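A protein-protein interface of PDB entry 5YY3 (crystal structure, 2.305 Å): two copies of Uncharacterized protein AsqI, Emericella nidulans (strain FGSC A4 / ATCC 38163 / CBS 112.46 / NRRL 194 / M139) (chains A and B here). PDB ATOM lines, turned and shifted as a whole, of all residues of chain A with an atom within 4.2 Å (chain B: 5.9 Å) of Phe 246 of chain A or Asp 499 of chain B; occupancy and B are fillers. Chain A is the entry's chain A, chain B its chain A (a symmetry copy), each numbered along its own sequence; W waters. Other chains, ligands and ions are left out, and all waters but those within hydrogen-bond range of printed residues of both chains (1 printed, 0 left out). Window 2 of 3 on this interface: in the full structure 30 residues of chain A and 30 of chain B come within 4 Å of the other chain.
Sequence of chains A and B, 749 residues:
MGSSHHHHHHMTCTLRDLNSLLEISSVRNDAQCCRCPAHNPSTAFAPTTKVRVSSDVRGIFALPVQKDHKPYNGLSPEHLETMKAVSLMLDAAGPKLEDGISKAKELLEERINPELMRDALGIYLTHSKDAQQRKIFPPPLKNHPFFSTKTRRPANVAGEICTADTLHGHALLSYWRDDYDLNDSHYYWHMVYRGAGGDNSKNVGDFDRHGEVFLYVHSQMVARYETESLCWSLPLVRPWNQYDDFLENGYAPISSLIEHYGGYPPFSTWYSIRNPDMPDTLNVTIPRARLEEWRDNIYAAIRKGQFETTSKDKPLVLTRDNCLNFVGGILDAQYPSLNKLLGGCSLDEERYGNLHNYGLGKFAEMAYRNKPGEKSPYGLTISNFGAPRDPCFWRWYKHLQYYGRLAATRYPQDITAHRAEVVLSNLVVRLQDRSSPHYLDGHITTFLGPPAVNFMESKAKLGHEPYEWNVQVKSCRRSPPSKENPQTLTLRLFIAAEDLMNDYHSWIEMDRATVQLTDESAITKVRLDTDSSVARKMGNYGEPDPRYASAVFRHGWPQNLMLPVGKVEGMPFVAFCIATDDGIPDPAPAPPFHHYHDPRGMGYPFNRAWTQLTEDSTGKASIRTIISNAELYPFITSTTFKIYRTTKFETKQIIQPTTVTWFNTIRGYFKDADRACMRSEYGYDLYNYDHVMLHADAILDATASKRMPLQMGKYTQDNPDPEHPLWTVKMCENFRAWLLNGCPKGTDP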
ATOM      1  N   ARG A 238      -9.837  12.499 -18.012  1.00  0.00           N
ATOM      2  CA  ARG A 238      -9.354  13.668 -18.749  1.00  0.00           C
ATOM      3  C   ARG A 238     -10.175  13.818 -20.020  1.00  0.00           C
ATOM      4  O   ARG A 238     -10.131  12.959 -20.893  1.00  0.00           O
ATOM      5  CB  ARG A 238      -7.869  13.554 -19.090  1.00  0.00           C
ATOM      6  CG  ARG A 238      -7.246  14.883 -19.577  1.00  0.00           C
ATOM      7  CD  ARG A 238      -5.896  14.667 -20.300  1.00  0.00           C
ATOM      8  NE  ARG A 238      -5.182  13.567 -19.677  1.00  0.00           N
ATOM      9  CZ  ARG A 238      -4.419  12.683 -20.307  1.00  0.00           C
ATOM     10  NH1 ARG A 238      -4.226  12.737 -21.618  1.00  0.00           N
ATOM     11  NH2 ARG A 238      -3.839  11.733 -19.598  1.00  0.00           N
ATOM     12  N   ASP A 244      -4.883  17.288 -29.891  1.00  0.00           N
ATOM     13  CA  ASP A 244      -3.534  16.774 -30.085  1.00  0.00           C
ATOM     14  C   ASP A 244      -3.079  15.977 -28.870  1.00  0.00           C
ATOM     15  O   ASP A 244      -1.891  15.899 -28.566  1.00  0.00           O
ATOM     16  CB  ASP A 244      -2.561  17.921 -30.354  1.00  0.00           C
ATOM     17  CG  ASP A 244      -2.565  18.951 -29.238  1.00  0.00           C
ATOM     18  OD1 ASP A 244      -3.544  18.966 -28.450  1.00  0.00           O
ATOM     19  OD2 ASP A 244      -1.606  19.756 -29.154  1.00  0.00           O
ATOM     20  N   ASP A 245      -4.033  15.384 -28.169  1.00  0.00           N
ATOM     21  CA  ASP A 245      -3.714  14.705 -26.923  1.00  0.00           C
ATOM     22  C   ASP A 245      -3.259  13.268 -27.168  1.00  0.00           C
ATOM     23  O   ASP A 245      -3.444  12.699 -28.256  1.00  0.00           O
ATOM     24  CB  ASP A 245      -4.919  14.722 -25.983  1.00  0.00           C
ATOM     25  CG  ASP A 245      -4.530  14.595 -24.523  1.00  0.00           C
ATOM     26  OD1 ASP A 245      -3.329  14.352 -24.250  1.00  0.00           O
ATOM     27  OD2 ASP A 245      -5.429  14.726 -23.654  1.00  0.00           O
ATOM     28  N   PHE A 246      -2.653  12.693 -26.137  1.00  0.00           N
ATOM     29  CA  PHE A 246      -2.246  11.312 -26.180  1.00  0.00           C
ATOM     30  C   PHE A 246      -3.250  10.449 -25.437  1.00  0.00           C
ATOM     31  O   PHE A 246      -3.877  10.894 -24.490  1.00  0.00           O
ATOM     32  CB  PHE A 246      -0.859  11.146 -25.568  1.00  0.00           C
ATOM     33  CG  PHE A 246       0.248  11.785 -26.369  1.00  0.00           C
ATOM     34  CD1 PHE A 246       0.841  11.105 -27.424  1.00  0.00           C
ATOM     35  CD2 PHE A 246       0.735  13.034 -26.030  1.00  0.00           C
ATOM     36  CE1 PHE A 246       1.879  11.679 -28.159  1.00  0.00           C
ATOM     37  CE2 PHE A 246       1.782  13.613 -26.749  1.00  0.00           C
ATOM     38  CZ  PHE A 246       2.351  12.934 -27.816  1.00  0.00           C
ATOM     39  N   LEU A 247      -3.409   9.216 -25.890  1.00  0.00           N
ATOM     40  CA  LEU A 247      -4.071   8.182 -25.118  1.00  0.00           C
ATOM     41  C   LEU A 247      -2.984   7.321 -24.469  1.00  0.00           C
ATOM     42  O   LEU A 247      -2.506   6.367 -25.070  1.00  0.00           O
ATOM     43  CB  LEU A 247      -4.968   7.342 -26.022  1.00  0.00           C
ATOM     44  CG  LEU A 247      -6.236   8.014 -26.554  1.00  0.00           C
ATOM     45  CD1 LEU A 247      -6.700   7.318 -27.799  1.00  0.00           C
ATOM     46  CD2 LEU A 247      -7.322   7.966 -25.494  1.00  0.00           C
ATOM     47  N   GLU A 248      -2.585   7.641 -23.247  1.00  0.00           N
ATOM     48  CA  GLU A 248      -1.351   7.057 -22.736  1.00  0.00           C
ATOM     49  C   GLU A 248      -1.431   5.586 -22.300  1.00  0.00           C
ATOM     50  O   GLU A 248      -0.388   4.961 -22.092  1.00  0.00           O
ATOM     51  CB  GLU A 248      -0.822   7.902 -21.573  1.00  0.00           C
ATOM     52  CG  GLU A 248      -1.743   7.986 -20.385  1.00  0.00           C
ATOM     53  CD  GLU A 248      -2.398   9.351 -20.268  1.00  0.00           C
ATOM     54  OE1 GLU A 248      -2.975   9.814 -21.278  1.00  0.00           O
ATOM     55  OE2 GLU A 248      -2.344   9.961 -19.170  1.00  0.00           O
ATOM     56  N   PHE A 267      -0.061   5.688 -25.901  1.00  0.00           N
ATOM     57  CA  PHE A 267       0.307   6.957 -26.529  1.00  0.00           C
ATOM     58  C   PHE A 267      -0.051   7.028 -28.015  1.00  0.00           C
ATOM     59  O   PHE A 267       0.639   7.665 -28.793  1.00  0.00           O
ATOM     60  CB  PHE A 267       1.801   7.234 -26.309  1.00  0.00           C
ATOM     61  CG  PHE A 267       2.158   7.416 -24.857  1.00  0.00           C
ATOM     62  CD1 PHE A 267       2.477   6.322 -24.064  1.00  0.00           C
ATOM     63  CD2 PHE A 267       2.134   8.675 -24.274  1.00  0.00           C
ATOM     64  CE1 PHE A 267       2.783   6.477 -22.711  1.00  0.00           C
ATOM     65  CE2 PHE A 267       2.448   8.838 -22.931  1.00  0.00           C
ATOM     66  CZ  PHE A 267       2.767   7.733 -22.142  1.00  0.00           C
ATOM     67  N   SER A 268      -1.148   6.387 -28.396  1.00  0.00           N
ATOM     68  CA  SER A 268      -1.766   6.633 -29.700  1.00  0.00           C
ATOM     69  C   SER A 268      -2.340   8.042 -29.744  1.00  0.00           C
ATOM     70  O   SER A 268      -2.650   8.624 -28.701  1.00  0.00           O
ATOM     71  CB  SER A 268      -2.870   5.601 -29.979  1.00  0.00           C
ATOM     72  OG  SER A 268      -2.319   4.288 -30.044  1.00  0.00           O
ATOM     73  N   THR A 269      -2.467   8.604 -30.941  1.00  0.00           N
ATOM     74  CA  THR A 269      -3.078   9.924 -31.118  1.00  0.00           C
ATOM     75  C   THR A 269      -3.967   9.936 -32.344  1.00  0.00           C
ATOM     76  O   THR A 269      -3.938   9.000 -33.143  1.00  0.00           O
ATOM     77  CB  THR A 269      -2.041  11.042 -31.316  1.00  0.00           C
ATOM     78  OG1 THR A 269      -1.409  10.876 -32.598  1.00  0.00           O
ATOM     79  CG2 THR A 269      -1.002  11.036 -30.215  1.00  0.00           C
ATOM     80  N   ARG A 395     -13.438   9.516 -23.046  1.00  0.00           N
ATOM     81  CA  ARG A 395     -12.778  10.818 -23.068  1.00  0.00           C
ATOM     82  C   ARG A 395     -13.492  11.739 -24.072  1.00  0.00           C
ATOM     83  O   ARG A 395     -13.627  12.942 -23.833  1.00  0.00           O
ATOM     84  CB  ARG A 395     -11.282  10.676 -23.387  1.00  0.00           C
ATOM     85  CG  ARG A 395     -10.521   9.801 -22.362  1.00  0.00           C
ATOM     86  CD  ARG A 395      -8.991  10.009 -22.435  1.00  0.00           C
ATOM     87  NE  ARG A 395      -8.734  11.435 -22.527  1.00  0.00           N
ATOM     88  CZ  ARG A 395      -7.577  11.975 -22.878  1.00  0.00           C
ATOM     89  NH1 ARG A 395      -6.529  11.194 -23.147  1.00  0.00           N
ATOM     90  NH2 ARG A 395      -7.480  13.303 -22.955  1.00  0.00           N
ATOM     91  N   LEU B 230       5.875  10.738 -16.537  1.00  0.00           N
ATOM     92  CA  LEU B 230       5.927   9.527 -17.334  1.00  0.00           C
ATOM     93  C   LEU B 230       7.017   8.569 -16.868  1.00  0.00           C
ATOM     94  O   LEU B 230       6.901   7.352 -17.035  1.00  0.00           O
ATOM     95  CB  LEU B 230       6.154   9.877 -18.802  1.00  0.00           C
ATOM     96  CG  LEU B 230       4.955   9.705 -19.727  1.00  0.00           C
ATOM     97  CD1 LEU B 230       3.718  10.229 -19.055  1.00  0.00           C
ATOM     98  CD2 LEU B 230       5.209  10.439 -21.030  1.00  0.00           C
ATOM     99  N   LEU B 236      -0.545  11.723 -17.115  1.00  0.00           N
ATOM    100  CA  LEU B 236      -0.294  13.070 -17.582  1.00  0.00           C
ATOM    101  C   LEU B 236      -1.202  14.015 -16.792  1.00  0.00           C
ATOM    102  O   LEU B 236      -2.206  13.592 -16.207  1.00  0.00           O
ATOM    103  CB  LEU B 236      -0.547  13.178 -19.088  1.00  0.00           C
ATOM    104  CG  LEU B 236       0.394  12.455 -20.066  1.00  0.00           C
ATOM    105  CD1 LEU B 236      -0.164  12.495 -21.488  1.00  0.00           C
ATOM    106  CD2 LEU B 236       1.810  13.024 -20.036  1.00  0.00           C
ATOM    107  N   ALA B 496      13.126  14.771 -25.970  1.00  0.00           N
ATOM    108  CA  ALA B 496      11.738  14.422 -25.760  1.00  0.00           C
ATOM    109  C   ALA B 496      11.660  12.946 -25.403  1.00  0.00           C
ATOM    110  O   ALA B 496      12.379  12.129 -25.977  1.00  0.00           O
ATOM    111  CB  ALA B 496      10.917  14.721 -26.988  1.00  0.00           C
ATOM    112  N   ALA B 497      10.831  12.620 -24.414  1.00  0.00           N
ATOM    113  CA  ALA B 497      10.466  11.232 -24.153  1.00  0.00           C
ATOM    114  C   ALA B 497       9.974  10.632 -25.464  1.00  0.00           C
ATOM    115  O   ALA B 497       9.161  11.249 -26.159  1.00  0.00           O
ATOM    116  CB  ALA B 497       9.377  11.142 -23.053  1.00  0.00           C
ATOM    117  N   GLU B 498      10.467   9.448 -25.813  1.00  0.00           N
ATOM    118  CA  GLU B 498      10.129   8.850 -27.106  1.00  0.00           C
ATOM    119  C   GLU B 498       8.612   8.785 -27.384  1.00  0.00           C
ATOM    120  O   GLU B 498       8.187   8.935 -28.525  1.00  0.00           O
ATOM    121  CB  GLU B 498      10.735   7.452 -27.211  1.00  0.00           C
ATOM    122  CG  GLU B 498      10.696   6.877 -28.639  1.00  0.00           C
ATOM    123  CD  GLU B 498      11.488   5.571 -28.794  1.00  0.00           C
ATOM    124  OE1 GLU B 498      12.653   5.517 -28.342  1.00  0.00           O
ATOM    125  OE2 GLU B 498      10.951   4.600 -29.373  1.00  0.00           O
ATOM    126  N   ASP B 499       7.801   8.562 -26.352  1.00  0.00           N
ATOM    127  CA  ASP B 499       6.346   8.480 -26.535  1.00  0.00           C
ATOM    128  C   ASP B 499       5.722   9.826 -26.892  1.00  0.00           C
ATOM    129  O   ASP B 499       4.730   9.883 -27.627  1.00  0.00           O
ATOM    130  CB  ASP B 499       5.663   7.932 -25.271  1.00  0.00           C
ATOM    131  CG  ASP B 499       5.970   6.467 -25.036  1.00  0.00           C
ATOM    132  OD1 ASP B 499       6.099   5.732 -26.037  1.00  0.00           O
ATOM    133  OD2 ASP B 499       6.085   6.051 -23.855  1.00  0.00           O
ATOM    134  N   LEU B 500       6.292  10.906 -26.364  1.00  0.00           N
ATOM    135  CA  LEU B 500       5.723  12.240 -26.576  1.00  0.00           C
ATOM    136  C   LEU B 500       6.312  12.958 -27.788  1.00  0.00           C
ATOM    137  O   LEU B 500       5.920  14.071 -28.109  1.00  0.00           O
ATOM    138  CB  LEU B 500       5.934  13.108 -25.334  1.00  0.00           C
ATOM    139  CG  LEU B 500       5.504  12.551 -23.983  1.00  0.00           C
ATOM    140  CD1 LEU B 500       5.809  13.544 -22.876  1.00  0.00           C
ATOM    141  CD2 LEU B 500       4.031  12.216 -24.017  1.00  0.00           C
ATOM    142  N   MET B 501       7.257  12.303 -28.454  1.00  0.00           N
ATOM    143  CA  MET B 501       8.088  12.918 -29.492  1.00  0.00           C
ATOM    144  C   MET B 501       7.350  13.656 -30.617  1.00  0.00           C
ATOM    145  O   MET B 501       7.885  14.621 -31.164  1.00  0.00           O
ATOM    146  CB  MET B 501       8.991  11.812 -30.062  1.00  0.00           C
ATOM    147  CG  MET B 501       9.617  12.048 -31.389  1.00  0.00           C
ATOM    148  SD  MET B 501      10.412  10.533 -31.953  1.00  0.00           S
ATOM    149  CE  MET B 501       9.217   9.357 -31.410  1.00  0.00           C
ATOM    150  N   ASN B 502       6.128  13.247 -30.960  1.00  0.00           N
ATOM    151  CA  ASN B 502       5.399  13.937 -32.038  1.00  0.00           C
ATOM    152  C   ASN B 502       4.552  15.133 -31.591  1.00  0.00           C
ATOM    153  O   ASN B 502       3.798  15.698 -32.378  1.00  0.00           O
ATOM    154  CB  ASN B 502       4.500  12.960 -32.785  1.00  0.00           C
ATOM    155  CG  ASN B 502       5.278  12.031 -33.665  1.00  0.00           C
ATOM    156  OD1 ASN B 502       6.346  12.388 -34.190  1.00  0.00           O
ATOM    157  ND2 ASN B 502       4.762  10.827 -33.838  1.00  0.00           N
ATOM    158  N   ASP B 503       4.660  15.492 -30.323  1.00  0.00           N
ATOM    159  CA  ASP B 503       4.035  16.696 -29.819  1.00  0.00           C
ATOM    160  C   ASP B 503       5.099  17.772 -29.705  1.00  0.00           C
ATOM    161  O   ASP B 503       6.053  17.617 -28.932  1.00  0.00           O
ATOM    162  CB  ASP B 503       3.380  16.431 -28.461  1.00  0.00           C
ATOM    163  CG  ASP B 503       2.871  17.686 -27.801  1.00  0.00           C
ATOM    164  OD1 ASP B 503       2.486  18.630 -28.528  1.00  0.00           O
ATOM    165  OD2 ASP B 503       2.842  17.725 -26.549  1.00  0.00           O
ATOM    166  N   SER B 506       6.075  19.000 -26.253  1.00  0.00           N
ATOM    167  CA  SER B 506       6.706  18.044 -25.349  1.00  0.00           C
ATOM    168  C   SER B 506       8.223  18.085 -25.464  1.00  0.00           C
ATOM    169  O   SER B 506       8.929  17.470 -24.659  1.00  0.00           O
ATOM    170  CB  SER B 506       6.203  16.632 -25.618  1.00  0.00           C
ATOM    171  OG  SER B 506       4.863  16.486 -25.165  1.00  0.00           O
ATOM    172  N   PRO B 572      13.872   5.432 -22.917  1.00  0.00           N
ATOM    173  CA  PRO B 572      14.285   5.966 -24.223  1.00  0.00           C
ATOM    174  C   PRO B 572      13.840   7.410 -24.461  1.00  0.00           C
ATOM    175  O   PRO B 572      12.678   7.761 -24.270  1.00  0.00           O
ATOM    176  CB  PRO B 572      13.627   4.997 -25.227  1.00  0.00           C
ATOM    177  CG  PRO B 572      12.521   4.354 -24.485  1.00  0.00           C
ATOM    178  CD  PRO B 572      12.919   4.314 -23.034  1.00  0.00           C
HETATM  179  O   HOH W   1      -5.220  13.032 -16.943  1.00  0.00           O
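OE2 of Glu 248 of chain A lies within hydrogen-bond range of N of Leu 236 of chain B (3.3 Å).
The side-chain carboxylate (OD2) of Asp 245 of chain A is in salt-bridge range of the guanidinium group (NH1) of Arg 238 of chain A.
The guanidinium group of Arg 238 of chain A sits at hydrogen-bond distance from the backbone carbonyl oxygen of Phe 246 of chain A (3.4 Å).
The side-chain hydroxyl (OG) of Ser 506 of chain B is in hydrogen-bond range of the side-chain carboxylate (OD2) of Asp 503 of chain B.
The backbone carbonyl oxygen (O) of Arg 238 of chain A is in hydrogen-bond range of the guanidinium group (NE) of Arg 395 of chain A (2.6 Å).
The backbone carbonyl oxygen (O) of Phe 246 of chain A is in hydrogen-bond range of the guanidinium group (NH1) of Arg 395 of chain A (3.0 Å).
The guanidinium group of Arg 238 of chain A lies within salt-bridge range of the side-chain carboxylate of Glu 248 of chain A, at 2.7 Å.
Leu 236 of chain B touches Arg 238 of chain A.
Phe 246 of chain A touches Asp 499 of chain B.
Phe 246 of chain A touches Leu 500 of chain B.
CB of Asp 503 of chain B touches CE2 of Phe 246 of chain A, 3.7 Å away.
Phe 267 of chain A touches Leu 230 of chain B (CE2 to CD2, 3.7 Å).
OD2 of Asp 499 of chain B touches CE1 of Phe 267 of chain A (3.5 Å).
Phe 267 of chain A touches Leu 500 of chain B (CE2 to CD2, 3.9 Å).
Printed residues of chain B within 4 Å of Arg 238 of chain A: Leu 236.
Asp 245 of chain A touches none of the printed residues of chain B.
Of the printed residues of chain B, Phe 246 of chain A touches Asp 499, Leu 500 and Asp 503.
Of the printed residues of chain A, Leu 236 of chain B touches Arg 238 (3.6 Å) and Glu 248 (3.3 Å).
Of the printed residues of chain A, Asp 499 of chain B touches Phe 246 (3.4 Å) and Phe 267 (3.5 Å).
Printed residues of chain A within 4 Å of Asp 503 of chain B: Phe 246 (3.7 Å).
Of the 12 printed residues of chain B, 5 touch a printed residue of chain A.
Hydrophobic or aromatic side chains of chain B that line the printed part of chain A: Leu 230, Leu 236 and Leu 500.
Of the 10 printed residues of chain A, 4 touch a printed residue of chain B.
Among the printed residues, 8 pairs touch across the chains.
Among the printed residues, no Asp or Glu carboxylate lies within 4 Å of a Lys or Arg side-chain nitrogen of the other chain.
No position is printed for both chains.
Of the 8 pairs that touch across the chains among the printed residues, none has its exchanged pair printed and touching as well.
Water W1 lies within hydrogen-bond range of the guanidinium group of Arg 238 of chain A (2.8 Å) and the backbone carbonyl oxygen of Leu 236 of chain B (3.2 Å).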
